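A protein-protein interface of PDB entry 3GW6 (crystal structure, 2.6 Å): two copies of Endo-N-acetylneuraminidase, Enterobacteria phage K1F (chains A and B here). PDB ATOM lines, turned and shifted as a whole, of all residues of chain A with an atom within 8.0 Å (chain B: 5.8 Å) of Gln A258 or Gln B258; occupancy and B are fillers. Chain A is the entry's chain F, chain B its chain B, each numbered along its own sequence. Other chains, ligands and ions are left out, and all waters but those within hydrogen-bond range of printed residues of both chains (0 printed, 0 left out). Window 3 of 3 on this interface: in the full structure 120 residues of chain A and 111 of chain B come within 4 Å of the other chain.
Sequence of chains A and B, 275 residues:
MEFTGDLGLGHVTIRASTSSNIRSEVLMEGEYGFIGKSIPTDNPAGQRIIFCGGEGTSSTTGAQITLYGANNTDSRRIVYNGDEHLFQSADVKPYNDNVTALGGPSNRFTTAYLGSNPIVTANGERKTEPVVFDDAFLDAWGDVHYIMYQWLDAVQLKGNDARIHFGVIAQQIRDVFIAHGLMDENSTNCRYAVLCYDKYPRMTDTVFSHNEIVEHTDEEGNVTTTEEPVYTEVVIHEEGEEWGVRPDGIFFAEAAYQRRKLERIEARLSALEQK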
ATOM      1  N   LEU A 138      18.930 -16.032 -15.037  1.00  0.00           N
ATOM      2  CA  LEU A 138      18.770 -16.596 -13.702  1.00  0.00           C
ATOM      3  C   LEU A 138      17.743 -15.805 -12.900  1.00  0.00           C
ATOM      4  O   LEU A 138      16.931 -16.380 -12.174  1.00  0.00           O
ATOM      5  CB  LEU A 138      20.112 -16.621 -12.969  1.00  0.00           C
ATOM      6  CG  LEU A 138      20.938 -17.905 -13.070  1.00  0.00           C
ATOM      7  CD1 LEU A 138      20.593 -18.680 -14.332  1.00  0.00           C
ATOM      8  CD2 LEU A 138      22.424 -17.581 -13.028  1.00  0.00           C
ATOM      9  N   TRP A 141      14.387 -16.974 -14.029  1.00  0.00           N
ATOM     10  CA  TRP A 141      14.173 -18.378 -13.696  1.00  0.00           C
ATOM     11  C   TRP A 141      13.618 -18.574 -12.286  1.00  0.00           C
ATOM     12  O   TRP A 141      12.954 -19.571 -12.006  1.00  0.00           O
ATOM     13  CB  TRP A 141      15.470 -19.172 -13.872  1.00  0.00           C
ATOM     14  CG  TRP A 141      15.245 -20.643 -13.962  1.00  0.00           C
ATOM     15  CD1 TRP A 141      15.631 -21.591 -13.059  1.00  0.00           C
ATOM     16  CD2 TRP A 141      14.563 -21.342 -15.016  1.00  0.00           C
ATOM     17  NE1 TRP A 141      15.239 -22.837 -13.487  1.00  0.00           N
ATOM     18  CE2 TRP A 141      14.586 -22.712 -14.675  1.00  0.00           C
ATOM     19  CE3 TRP A 141      13.946 -20.943 -16.200  1.00  0.00           C
ATOM     20  CZ2 TRP A 141      14.007 -23.683 -15.497  1.00  0.00           C
ATOM     21  CZ3 TRP A 141      13.374 -21.912 -17.009  1.00  0.00           C
ATOM     22  CH2 TRP A 141      13.409 -23.264 -16.653  1.00  0.00           C
ATOM     23  N   TYR A 146       7.489 -24.805  -9.445  1.00  0.00           N
ATOM     24  CA  TYR A 146       7.383 -26.252  -9.495  1.00  0.00           C
ATOM     25  C   TYR A 146       6.131 -26.683  -8.750  1.00  0.00           C
ATOM     26  O   TYR A 146       5.989 -26.422  -7.555  1.00  0.00           O
ATOM     27  CB  TYR A 146       8.639 -26.892  -8.911  1.00  0.00           C
ATOM     28  CG  TYR A 146       9.874 -26.574  -9.721  1.00  0.00           C
ATOM     29  CD1 TYR A 146      10.208 -27.337 -10.832  1.00  0.00           C
ATOM     30  CD2 TYR A 146      10.694 -25.499  -9.393  1.00  0.00           C
ATOM     31  CE1 TYR A 146      11.328 -27.051 -11.586  1.00  0.00           C
ATOM     32  CE2 TYR A 146      11.820 -25.203 -10.143  1.00  0.00           C
ATOM     33  CZ  TYR A 146      12.130 -25.985 -11.239  1.00  0.00           C
ATOM     34  OH  TYR A 146      13.242 -25.708 -11.996  1.00  0.00           O
ATOM     35  N   PHE A 251      15.984 -28.567 -15.742  1.00  0.00           N
ATOM     36  CA  PHE A 251      16.899 -28.906 -14.657  1.00  0.00           C
ATOM     37  C   PHE A 251      18.304 -28.343 -14.875  1.00  0.00           C
ATOM     38  O   PHE A 251      18.987 -27.986 -13.918  1.00  0.00           O
ATOM     39  CB  PHE A 251      16.946 -30.422 -14.438  1.00  0.00           C
ATOM     40  CG  PHE A 251      15.590 -31.054 -14.298  1.00  0.00           C
ATOM     41  CD1 PHE A 251      14.666 -30.546 -13.400  1.00  0.00           C
ATOM     42  CD2 PHE A 251      15.241 -32.156 -15.060  1.00  0.00           C
ATOM     43  CE1 PHE A 251      13.415 -31.120 -13.269  1.00  0.00           C
ATOM     44  CE2 PHE A 251      13.992 -32.737 -14.934  1.00  0.00           C
ATOM     45  CZ  PHE A 251      13.078 -32.219 -14.037  1.00  0.00           C
ATOM     46  N   PHE A 252      18.735 -28.264 -16.129  1.00  0.00           N
ATOM     47  CA  PHE A 252      20.013 -27.636 -16.428  1.00  0.00           C
ATOM     48  C   PHE A 252      20.007 -26.195 -15.925  1.00  0.00           C
ATOM     49  O   PHE A 252      20.961 -25.740 -15.292  1.00  0.00           O
ATOM     50  CB  PHE A 252      20.300 -27.668 -17.928  1.00  0.00           C
ATOM     51  CG  PHE A 252      20.830 -28.984 -18.421  1.00  0.00           C
ATOM     52  CD1 PHE A 252      21.941 -29.563 -17.831  1.00  0.00           C
ATOM     53  CD2 PHE A 252      20.231 -29.630 -19.489  1.00  0.00           C
ATOM     54  CE1 PHE A 252      22.438 -30.771 -18.288  1.00  0.00           C
ATOM     55  CE2 PHE A 252      20.723 -30.838 -19.951  1.00  0.00           C
ATOM     56  CZ  PHE A 252      21.828 -31.408 -19.351  1.00  0.00           C
ATOM     57  N   ALA A 253      18.919 -25.486 -16.205  1.00  0.00           N
ATOM     58  CA  ALA A 253      18.772 -24.100 -15.775  1.00  0.00           C
ATOM     59  C   ALA A 253      18.620 -24.001 -14.260  1.00  0.00           C
ATOM     60  O   ALA A 253      19.158 -23.088 -13.634  1.00  0.00           O
ATOM     61  CB  ALA A 253      17.584 -23.450 -16.477  1.00  0.00           C
ATOM     62  N   GLU A 254      17.885 -24.943 -13.675  1.00  0.00           N
ATOM     63  CA  GLU A 254      17.673 -24.957 -12.231  1.00  0.00           C
ATOM     64  C   GLU A 254      18.967 -25.276 -11.490  1.00  0.00           C
ATOM     65  O   GLU A 254      19.168 -24.842 -10.359  1.00  0.00           O
ATOM     66  CB  GLU A 254      16.589 -25.967 -11.855  1.00  0.00           C
ATOM     67  CG  GLU A 254      16.216 -25.961 -10.381  1.00  0.00           C
ATOM     68  CD  GLU A 254      15.395 -24.750  -9.994  1.00  0.00           C
ATOM     69  OE1 GLU A 254      14.865 -24.074 -10.899  1.00  0.00           O
ATOM     70  OE2 GLU A 254      15.275 -24.472  -8.782  1.00  0.00           O
ATOM     71  N   ALA A 255      19.842 -26.036 -12.139  1.00  0.00           N
ATOM     72  CA  ALA A 255      21.137 -26.370 -11.560  1.00  0.00           C
ATOM     73  C   ALA A 255      22.064 -25.158 -11.588  1.00  0.00           C
ATOM     74  O   ALA A 255      22.917 -24.998 -10.719  1.00  0.00           O
ATOM     75  CB  ALA A 255      21.765 -27.545 -12.293  1.00  0.00           C
ATOM     76  N   ALA A 256      21.889 -24.310 -12.597  1.00  0.00           N
ATOM     77  CA  ALA A 256      22.668 -23.084 -12.713  1.00  0.00           C
ATOM     78  C   ALA A 256      22.128 -22.040 -11.743  1.00  0.00           C
ATOM     79  O   ALA A 256      22.887 -21.349 -11.062  1.00  0.00           O
ATOM     80  CB  ALA A 256      22.625 -22.563 -14.140  1.00  0.00           C
ATOM     81  N   TYR A 257      20.805 -21.936 -11.687  1.00  0.00           N
ATOM     82  CA  TYR A 257      20.135 -21.027 -10.769  1.00  0.00           C
ATOM     83  C   TYR A 257      20.567 -21.290  -9.332  1.00  0.00           C
ATOM     84  O   TYR A 257      21.186 -20.439  -8.692  1.00  0.00           O
ATOM     85  CB  TYR A 257      18.619 -21.182 -10.897  1.00  0.00           C
ATOM     86  CG  TYR A 257      17.811 -20.349  -9.927  1.00  0.00           C
ATOM     87  CD1 TYR A 257      17.815 -18.961  -9.998  1.00  0.00           C
ATOM     88  CD2 TYR A 257      17.024 -20.954  -8.952  1.00  0.00           C
ATOM     89  CE1 TYR A 257      17.068 -18.199  -9.118  1.00  0.00           C
ATOM     90  CE2 TYR A 257      16.274 -20.200  -8.069  1.00  0.00           C
ATOM     91  CZ  TYR A 257      16.298 -18.824  -8.158  1.00  0.00           C
ATOM     92  OH  TYR A 257      15.553 -18.070  -7.280  1.00  0.00           O
ATOM     93  N   GLN A 258      20.248 -22.481  -8.834  1.00  0.00           N
ATOM     94  CA  GLN A 258      20.530 -22.828  -7.446  1.00  0.00           C
ATOM     95  C   GLN A 258      22.021 -22.804  -7.110  1.00  0.00           C
ATOM     96  O   GLN A 258      22.392 -22.645  -5.949  1.00  0.00           O
ATOM     97  CB  GLN A 258      19.909 -24.181  -7.082  1.00  0.00           C
ATOM     98  CG  GLN A 258      18.387 -24.173  -7.086  1.00  0.00           C
ATOM     99  CD  GLN A 258      17.787 -25.386  -6.397  1.00  0.00           C
ATOM    100  OE1 GLN A 258      18.489 -26.155  -5.741  1.00  0.00           O
ATOM    101  NE2 GLN A 258      16.476 -25.559  -6.541  1.00  0.00           N
ATOM    102  N   ARG A 259      22.875 -22.954  -8.119  1.00  0.00           N
ATOM    103  CA  ARG A 259      24.313 -22.849  -7.890  1.00  0.00           C
ATOM    104  C   ARG A 259      24.737 -21.405  -7.630  1.00  0.00           C
ATOM    105  O   ARG A 259      25.580 -21.146  -6.772  1.00  0.00           O
ATOM    106  CB  ARG A 259      25.120 -23.448  -9.047  1.00  0.00           C
ATOM    107  CG  ARG A 259      25.301 -24.958  -8.961  1.00  0.00           C
ATOM    108  CD  ARG A 259      26.539 -25.422  -9.725  1.00  0.00           C
ATOM    109  NE  ARG A 259      26.648 -26.880  -9.757  1.00  0.00           N
ATOM    110  CZ  ARG A 259      27.748 -27.544 -10.101  1.00  0.00           C
ATOM    111  NH1 ARG A 259      28.852 -26.884 -10.437  1.00  0.00           N
ATOM    112  NH2 ARG A 259      27.748 -28.872 -10.104  1.00  0.00           N
ATOM    113  N   ARG A 260      24.156 -20.467  -8.374  1.00  0.00           N
ATOM    114  CA  ARG A 260      24.434 -19.053  -8.151  1.00  0.00           C
ATOM    115  C   ARG A 260      23.919 -18.633  -6.781  1.00  0.00           C
ATOM    116  O   ARG A 260      24.560 -17.855  -6.079  1.00  0.00           O
ATOM    117  CB  ARG A 260      23.799 -18.177  -9.235  1.00  0.00           C
ATOM    118  CG  ARG A 260      24.168 -16.703  -9.104  1.00  0.00           C
ATOM    119  CD  ARG A 260      23.410 -15.825 -10.083  1.00  0.00           C
ATOM    120  NE  ARG A 260      22.014 -15.651  -9.697  1.00  0.00           N
ATOM    121  CZ  ARG A 260      21.171 -14.824 -10.307  1.00  0.00           C
ATOM    122  NH1 ARG A 260      19.915 -14.728  -9.895  1.00  0.00           N
ATOM    123  NH2 ARG A 260      21.583 -14.092 -11.333  1.00  0.00           N
ATOM    124  N   LYS A 261      22.755 -19.153  -6.406  1.00  0.00           N
ATOM    125  CA  LYS A 261      22.155 -18.809  -5.125  1.00  0.00           C
ATOM    126  C   LYS A 261      23.029 -19.303  -3.976  1.00  0.00           C
ATOM    127  O   LYS A 261      23.389 -18.536  -3.086  1.00  0.00           O
ATOM    128  CB  LYS A 261      20.742 -19.383  -5.023  1.00  0.00           C
ATOM    129  CG  LYS A 261      19.790 -18.510  -4.226  1.00  0.00           C
ATOM    130  CD  LYS A 261      18.343 -18.929  -4.409  1.00  0.00           C
ATOM    131  CE  LYS A 261      17.402 -17.793  -4.035  1.00  0.00           C
ATOM    132  NZ  LYS A 261      16.094 -18.291  -3.528  1.00  0.00           N
ATOM    133  N   LEU A 262      23.371 -20.587  -4.008  1.00  0.00           N
ATOM    134  CA  LEU A 262      24.268 -21.177  -3.020  1.00  0.00           C
ATOM    135  C   LEU A 262      25.549 -20.364  -2.877  1.00  0.00           C
ATOM    136  O   LEU A 262      26.082 -20.209  -1.780  1.00  0.00           O
ATOM    137  CB  LEU A 262      24.614 -22.613  -3.414  1.00  0.00           C
ATOM    138  CG  LEU A 262      23.709 -23.718  -2.875  1.00  0.00           C
ATOM    139  CD1 LEU A 262      23.745 -24.939  -3.784  1.00  0.00           C
ATOM    140  CD2 LEU A 262      24.131 -24.078  -1.459  1.00  0.00           C
ATOM    141  N   GLU A 263      26.033 -19.840  -3.997  1.00  0.00           N
ATOM    142  CA  GLU A 263      27.263 -19.064  -4.012  1.00  0.00           C
ATOM    143  C   GLU A 263      27.073 -17.759  -3.247  1.00  0.00           C
ATOM    144  O   GLU A 263      27.887 -17.397  -2.394  1.00  0.00           O
ATOM    145  CB  GLU A 263      27.676 -18.783  -5.456  1.00  0.00           C
ATOM    146  CG  GLU A 263      29.173 -18.667  -5.675  1.00  0.00           C
ATOM    147  CD  GLU A 263      29.527 -18.478  -7.139  1.00  0.00           C
ATOM    148  OE2 GLU A 263      28.858 -17.666  -7.814  1.00  0.00           O
ATOM    149  N   ARG A 264      25.986 -17.062  -3.556  1.00  0.00           N
ATOM    150  CA  ARG A 264      25.665 -15.800  -2.903  1.00  0.00           C
ATOM    151  C   ARG A 264      25.396 -16.000  -1.415  1.00  0.00           C
ATOM    152  O   ARG A 264      25.689 -15.125  -0.601  1.00  0.00           O
ATOM    153  CB  ARG A 264      24.460 -15.148  -3.581  1.00  0.00           C
ATOM    154  CG  ARG A 264      24.716 -14.725  -5.017  1.00  0.00           C
ATOM    155  CD  ARG A 264      23.417 -14.389  -5.729  1.00  0.00           C
ATOM    156  NE  ARG A 264      23.647 -13.600  -6.934  1.00  0.00           N
ATOM    157  CZ  ARG A 264      22.678 -13.118  -7.706  1.00  0.00           C
ATOM    158  NH1 ARG A 264      21.406 -13.347  -7.403  1.00  0.00           N
ATOM    159  NH2 ARG A 264      22.977 -12.405  -8.784  1.00  0.00           N
ATOM    160  N   ILE A 265      24.835 -17.153  -1.066  1.00  0.00           N
ATOM    161  CA  ILE A 265      24.574 -17.487   0.331  1.00  0.00           C
ATOM    162  C   ILE A 265      25.871 -17.743   1.095  1.00  0.00           C
ATOM    163  O   ILE A 265      26.021 -17.319   2.242  1.00  0.00           O
ATOM    164  CB  ILE A 265      23.645 -18.715   0.464  1.00  0.00           C
ATOM    165  CG1 ILE A 265      22.178 -18.283   0.399  1.00  0.00           C
ATOM    166  CG2 ILE A 265      23.911 -19.451   1.769  1.00  0.00           C
ATOM    167  CD1 ILE A 265      21.197 -19.423   0.584  1.00  0.00           C
ATOM    168  N   ALA B 253      10.507 -32.722  -7.889  1.00  0.00           N
ATOM    169  CA  ALA B 253      10.307 -32.736  -6.444  1.00  0.00           C
ATOM    170  C   ALA B 253      11.541 -32.229  -5.704  1.00  0.00           C
ATOM    171  O   ALA B 253      11.426 -31.518  -4.708  1.00  0.00           O
ATOM    172  CB  ALA B 253       9.934 -34.137  -5.972  1.00  0.00           C
ATOM    173  N   GLU B 254      12.721 -32.603  -6.187  1.00  0.00           N
ATOM    174  CA  GLU B 254      13.964 -32.125  -5.593  1.00  0.00           C
ATOM    175  C   GLU B 254      14.044 -30.609  -5.734  1.00  0.00           C
ATOM    176  O   GLU B 254      14.449 -29.910  -4.806  1.00  0.00           O
ATOM    177  CB  GLU B 254      15.171 -32.788  -6.260  1.00  0.00           C
ATOM    178  CG  GLU B 254      16.512 -32.397  -5.659  1.00  0.00           C
ATOM    179  CD  GLU B 254      16.702 -32.938  -4.256  1.00  0.00           C
ATOM    180  OE1 GLU B 254      15.796 -33.643  -3.765  1.00  0.00           O
ATOM    181  OE2 GLU B 254      17.755 -32.661  -3.645  1.00  0.00           O
ATOM    182  N   ALA B 255      13.644 -30.110  -6.900  1.00  0.00           N
ATOM    183  CA  ALA B 255      13.612 -28.677  -7.156  1.00  0.00           C
ATOM    184  C   ALA B 255      12.746 -27.978  -6.116  1.00  0.00           C
ATOM    185  O   ALA B 255      13.204 -27.073  -5.419  1.00  0.00           O
ATOM    186  CB  ALA B 255      13.091 -28.401  -8.557  1.00  0.00           C
ATOM    187  N   ALA B 256      11.491 -28.404  -6.019  1.00  0.00           N
ATOM    188  CA  ALA B 256      10.572 -27.858  -5.031  1.00  0.00           C
ATOM    189  C   ALA B 256      11.182 -27.959  -3.640  1.00  0.00           C
ATOM    190  O   ALA B 256      11.132 -27.010  -2.857  1.00  0.00           O
ATOM    191  CB  ALA B 256       9.247 -28.595  -5.079  1.00  0.00           C
ATOM    192  N   TYR B 257      11.768 -29.115  -3.347  1.00  0.00           N
ATOM    193  CA  TYR B 257      12.394 -29.360  -2.058  1.00  0.00           C
ATOM    194  C   TYR B 257      13.449 -28.307  -1.742  1.00  0.00           C
ATOM    195  O   TYR B 257      13.314 -27.550  -0.781  1.00  0.00           O
ATOM    196  CB  TYR B 257      13.018 -30.757  -2.029  1.00  0.00           C
ATOM    197  CG  TYR B 257      13.828 -31.044  -0.783  1.00  0.00           C
ATOM    198  CD1 TYR B 257      13.218 -31.115   0.461  1.00  0.00           C
ATOM    199  CD2 TYR B 257      15.200 -31.251  -0.853  1.00  0.00           C
ATOM    200  CE1 TYR B 257      13.949 -31.377   1.602  1.00  0.00           C
ATOM    201  CE2 TYR B 257      15.940 -31.515   0.283  1.00  0.00           C
ATOM    202  CZ  TYR B 257      15.309 -31.576   1.508  1.00  0.00           C
ATOM    203  OH  TYR B 257      16.033 -31.839   2.645  1.00  0.00           O
ATOM    204  N   GLN B 258      14.495 -28.261  -2.558  1.00  0.00           N
ATOM    205  CA  GLN B 258      15.620 -27.368  -2.306  1.00  0.00           C
ATOM    206  C   GLN B 258      15.222 -25.894  -2.306  1.00  0.00           C
ATOM    207  O   GLN B 258      15.773 -25.100  -1.543  1.00  0.00           O
ATOM    208  CB  GLN B 258      16.752 -27.621  -3.303  1.00  0.00           C
ATOM    209  CG  GLN B 258      17.350 -29.016  -3.209  1.00  0.00           C
ATOM    210  CD  GLN B 258      18.779 -29.068  -3.710  1.00  0.00           C
ATOM    211  NE2 GLN B 258      19.307 -30.277  -3.873  1.00  0.00           N
ATOM    212  N   ARG B 259      14.266 -25.528  -3.155  1.00  0.00           N
ATOM    213  CA  ARG B 259      13.806 -24.144  -3.203  1.00  0.00           C
ATOM    214  C   ARG B 259      13.244 -23.703  -1.856  1.00  0.00           C
ATOM    215  O   ARG B 259      13.398 -22.547  -1.459  1.00  0.00           O
ATOM    216  CB  ARG B 259      12.777 -23.935  -4.318  1.00  0.00           C
ATOM    217  CG  ARG B 259      13.391 -23.847  -5.706  1.00  0.00           C
ATOM    218  CD  ARG B 259      12.544 -23.001  -6.643  1.00  0.00           C
ATOM    219  NE  ARG B 259      13.275 -22.647  -7.857  1.00  0.00           N
ATOM    220  CZ  ARG B 259      12.897 -21.705  -8.715  1.00  0.00           C
ATOM    221  NH1 ARG B 259      11.789 -21.010  -8.496  1.00  0.00           N
ATOM    222  NH2 ARG B 259      13.630 -21.455  -9.792  1.00  0.00           N
ATOM    223  N   ARG B 260      12.598 -24.625  -1.151  1.00  0.00           N
ATOM    224  CA  ARG B 260      12.099 -24.327   0.185  1.00  0.00           C
ATOM    225  C   ARG B 260      13.262 -24.231   1.163  1.00  0.00           C
ATOM    226  O   ARG B 260      13.312 -23.326   1.998  1.00  0.00           O
ATOM    227  CB  ARG B 260      11.099 -25.384   0.656  1.00  0.00           C
ATOM    228  CG  ARG B 260      10.359 -24.984   1.923  1.00  0.00           C
ATOM    229  CD  ARG B 260       9.493 -26.112   2.456  1.00  0.00           C
ATOM    230  NE  ARG B 260      10.291 -27.209   2.992  1.00  0.00           N
ATOM    231  CZ  ARG B 260       9.784 -28.242   3.658  1.00  0.00           C
ATOM    232  NH1 ARG B 260      10.582 -29.200   4.111  1.00  0.00           N
ATOM    233  NH2 ARG B 260       8.477 -28.316   3.871  1.00  0.00           N
ATOM    234  N   LYS B 261      14.203 -25.163   1.055  1.00  0.00           N
ATOM    235  CA  LYS B 261      15.381 -25.134   1.908  1.00  0.00           C
ATOM    236  C   LYS B 261      16.168 -23.847   1.672  1.00  0.00           C
ATOM    237  O   LYS B 261      16.898 -23.386   2.546  1.00  0.00           O
ATOM    238  CB  LYS B 261      16.256 -26.370   1.681  1.00  0.00           C
ATOM    239  CG  LYS B 261      17.415 -26.488   2.660  1.00  0.00           C
ATOM    240  CD  LYS B 261      17.890 -27.927   2.806  1.00  0.00           C
ATOM    241  CE  LYS B 261      16.932 -28.745   3.660  1.00  0.00           C
ATOM    242  NZ  LYS B 261      17.535 -30.036   4.097  1.00  0.00           N
ATOM    243  N   LEU B 262      16.002 -23.266   0.487  1.00  0.00           N
ATOM    244  CA  LEU B 262      16.634 -21.990   0.165  1.00  0.00           C
ATOM    245  C   LEU B 262      15.816 -20.812   0.687  1.00  0.00           C
ATOM    246  O   LEU B 262      16.373 -19.815   1.145  1.00  0.00           O
ATOM    247  CB  LEU B 262      16.864 -21.858  -1.343  1.00  0.00           C
ATOM    248  CG  LEU B 262      18.252 -22.275  -1.838  1.00  0.00           C
ATOM    249  CD1 LEU B 262      18.628 -23.652  -1.323  1.00  0.00           C
ATOM    250  CD2 LEU B 262      18.330 -22.230  -3.355  1.00  0.00           C
ATOM    251  N   GLU B 263      14.493 -20.928   0.613  1.00  0.00           N
ATOM    252  CA  GLU B 263      13.612 -19.904   1.157  1.00  0.00           C
ATOM    253  C   GLU B 263      13.880 -19.720   2.643  1.00  0.00           C
ATOM    254  O   GLU B 263      14.052 -18.601   3.124  1.00  0.00           O
ATOM    255  CB  GLU B 263      12.144 -20.283   0.939  1.00  0.00           C
ATOM    256  CG  GLU B 263      11.637 -20.057  -0.476  1.00  0.00           C
ATOM    257  CD  GLU B 263      11.541 -18.586  -0.834  1.00  0.00           C
ATOM    258  OE1 GLU B 263      11.655 -17.741   0.079  1.00  0.00           O
ATOM    259  OE2 GLU B 263      11.349 -18.274  -2.029  1.00  0.00           O
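The side-chain carboxylate of Glu B254 sits at hydrogen-bond distance from the side-chain amide nitrogen of Gln B258 (2.9 Å). NE1 of Trp A141 sits at hydrogen-bond distance from OE1 of Glu A254. OE1 of Glu A254 is in hydrogen-bond range of OH of Tyr A146 (2.6 Å). OE2 of Glu A254 lies within hydrogen-bond range of NE2 of Gln A258.
Of the printed residues of chain B, Glu A254 touches Arg B259 (2.9 Å). Ala A256 touches none of the printed residues of chain B. Gln A258 touches just these residues of chain B: Ala B255, Gln B258 and Arg B259. Printed residues of chain A within 4 Å of Ala B255: Tyr A146 (3.7 Å) and Gln A258 (3.8 Å). Of chain A, only Gln A258 (3.3 Å) comes within 4 Å of Gln B258. Of the printed residues of chain A, Leu B262 touches Lys A261 (3.5 Å). The nearest residue of chain B that does not touch Gln A258 is Leu B262 (4.2 Å). The nearest residue of chain A that does not touch Gln B258 is Leu A262 (6.5 Å).
Hydrophobic or aromatic side chains of chain A that line the printed part of chain B: Trp A141, Tyr A146 and Tyr A257. Along chain A the printed residues that touch a printed residue of chain B span positions 141 to 261. Printed residues of chain B that touch a printed residue of chain A: Ala B255, Gln B258, Arg B259 and Leu B262. Among the printed residues, 9 pairs touch across the chains. Among the printed residues, Asp or Glu carboxylates within 4 Å of a Lys or Arg side-chain nitrogen of the other chain: Glu A254 with Arg B259 (2.9 Å).
Among the printed residues, pairs that only touch across the chains: Gln A258 with Gln B258 (3.3 Å), Tyr A257 with Arg B259 (3.4 Å), Lys A261 with Leu B262 (3.5 Å), Gln A258 with Arg B259 (3.6 Å), Tyr A146 with Arg B259 (3.7 Å), Tyr A146 with Ala B255 (3.7 Å) and Gln A258 with Ala B255 (3.8 Å).
NH2 of Arg B259 is in hydrogen-bond range of O of Trp A141, 3.0 Å away. NE of Arg B259 lies within salt-bridge range of OE2 of Glu A254, 2.9 Å away.
Glu A254 touches Arg B259, but with the chains exchanged Arg A259 does not touch Glu B254 (11.4 Å). Gln A258 touches its own counterpart, Gln B258. Gln A258 touches Arg B259, but with the chains exchanged Arg A259 does not touch Gln B258 (8.6 Å). Lys A261 touches Leu B262, but with the chains exchanged Leu A262 does not touch Lys B261 (8.2 Å). Of the 9 pairs that touch across the chains among the printed residues, 1 has its exchanged pair printed and touching as well.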
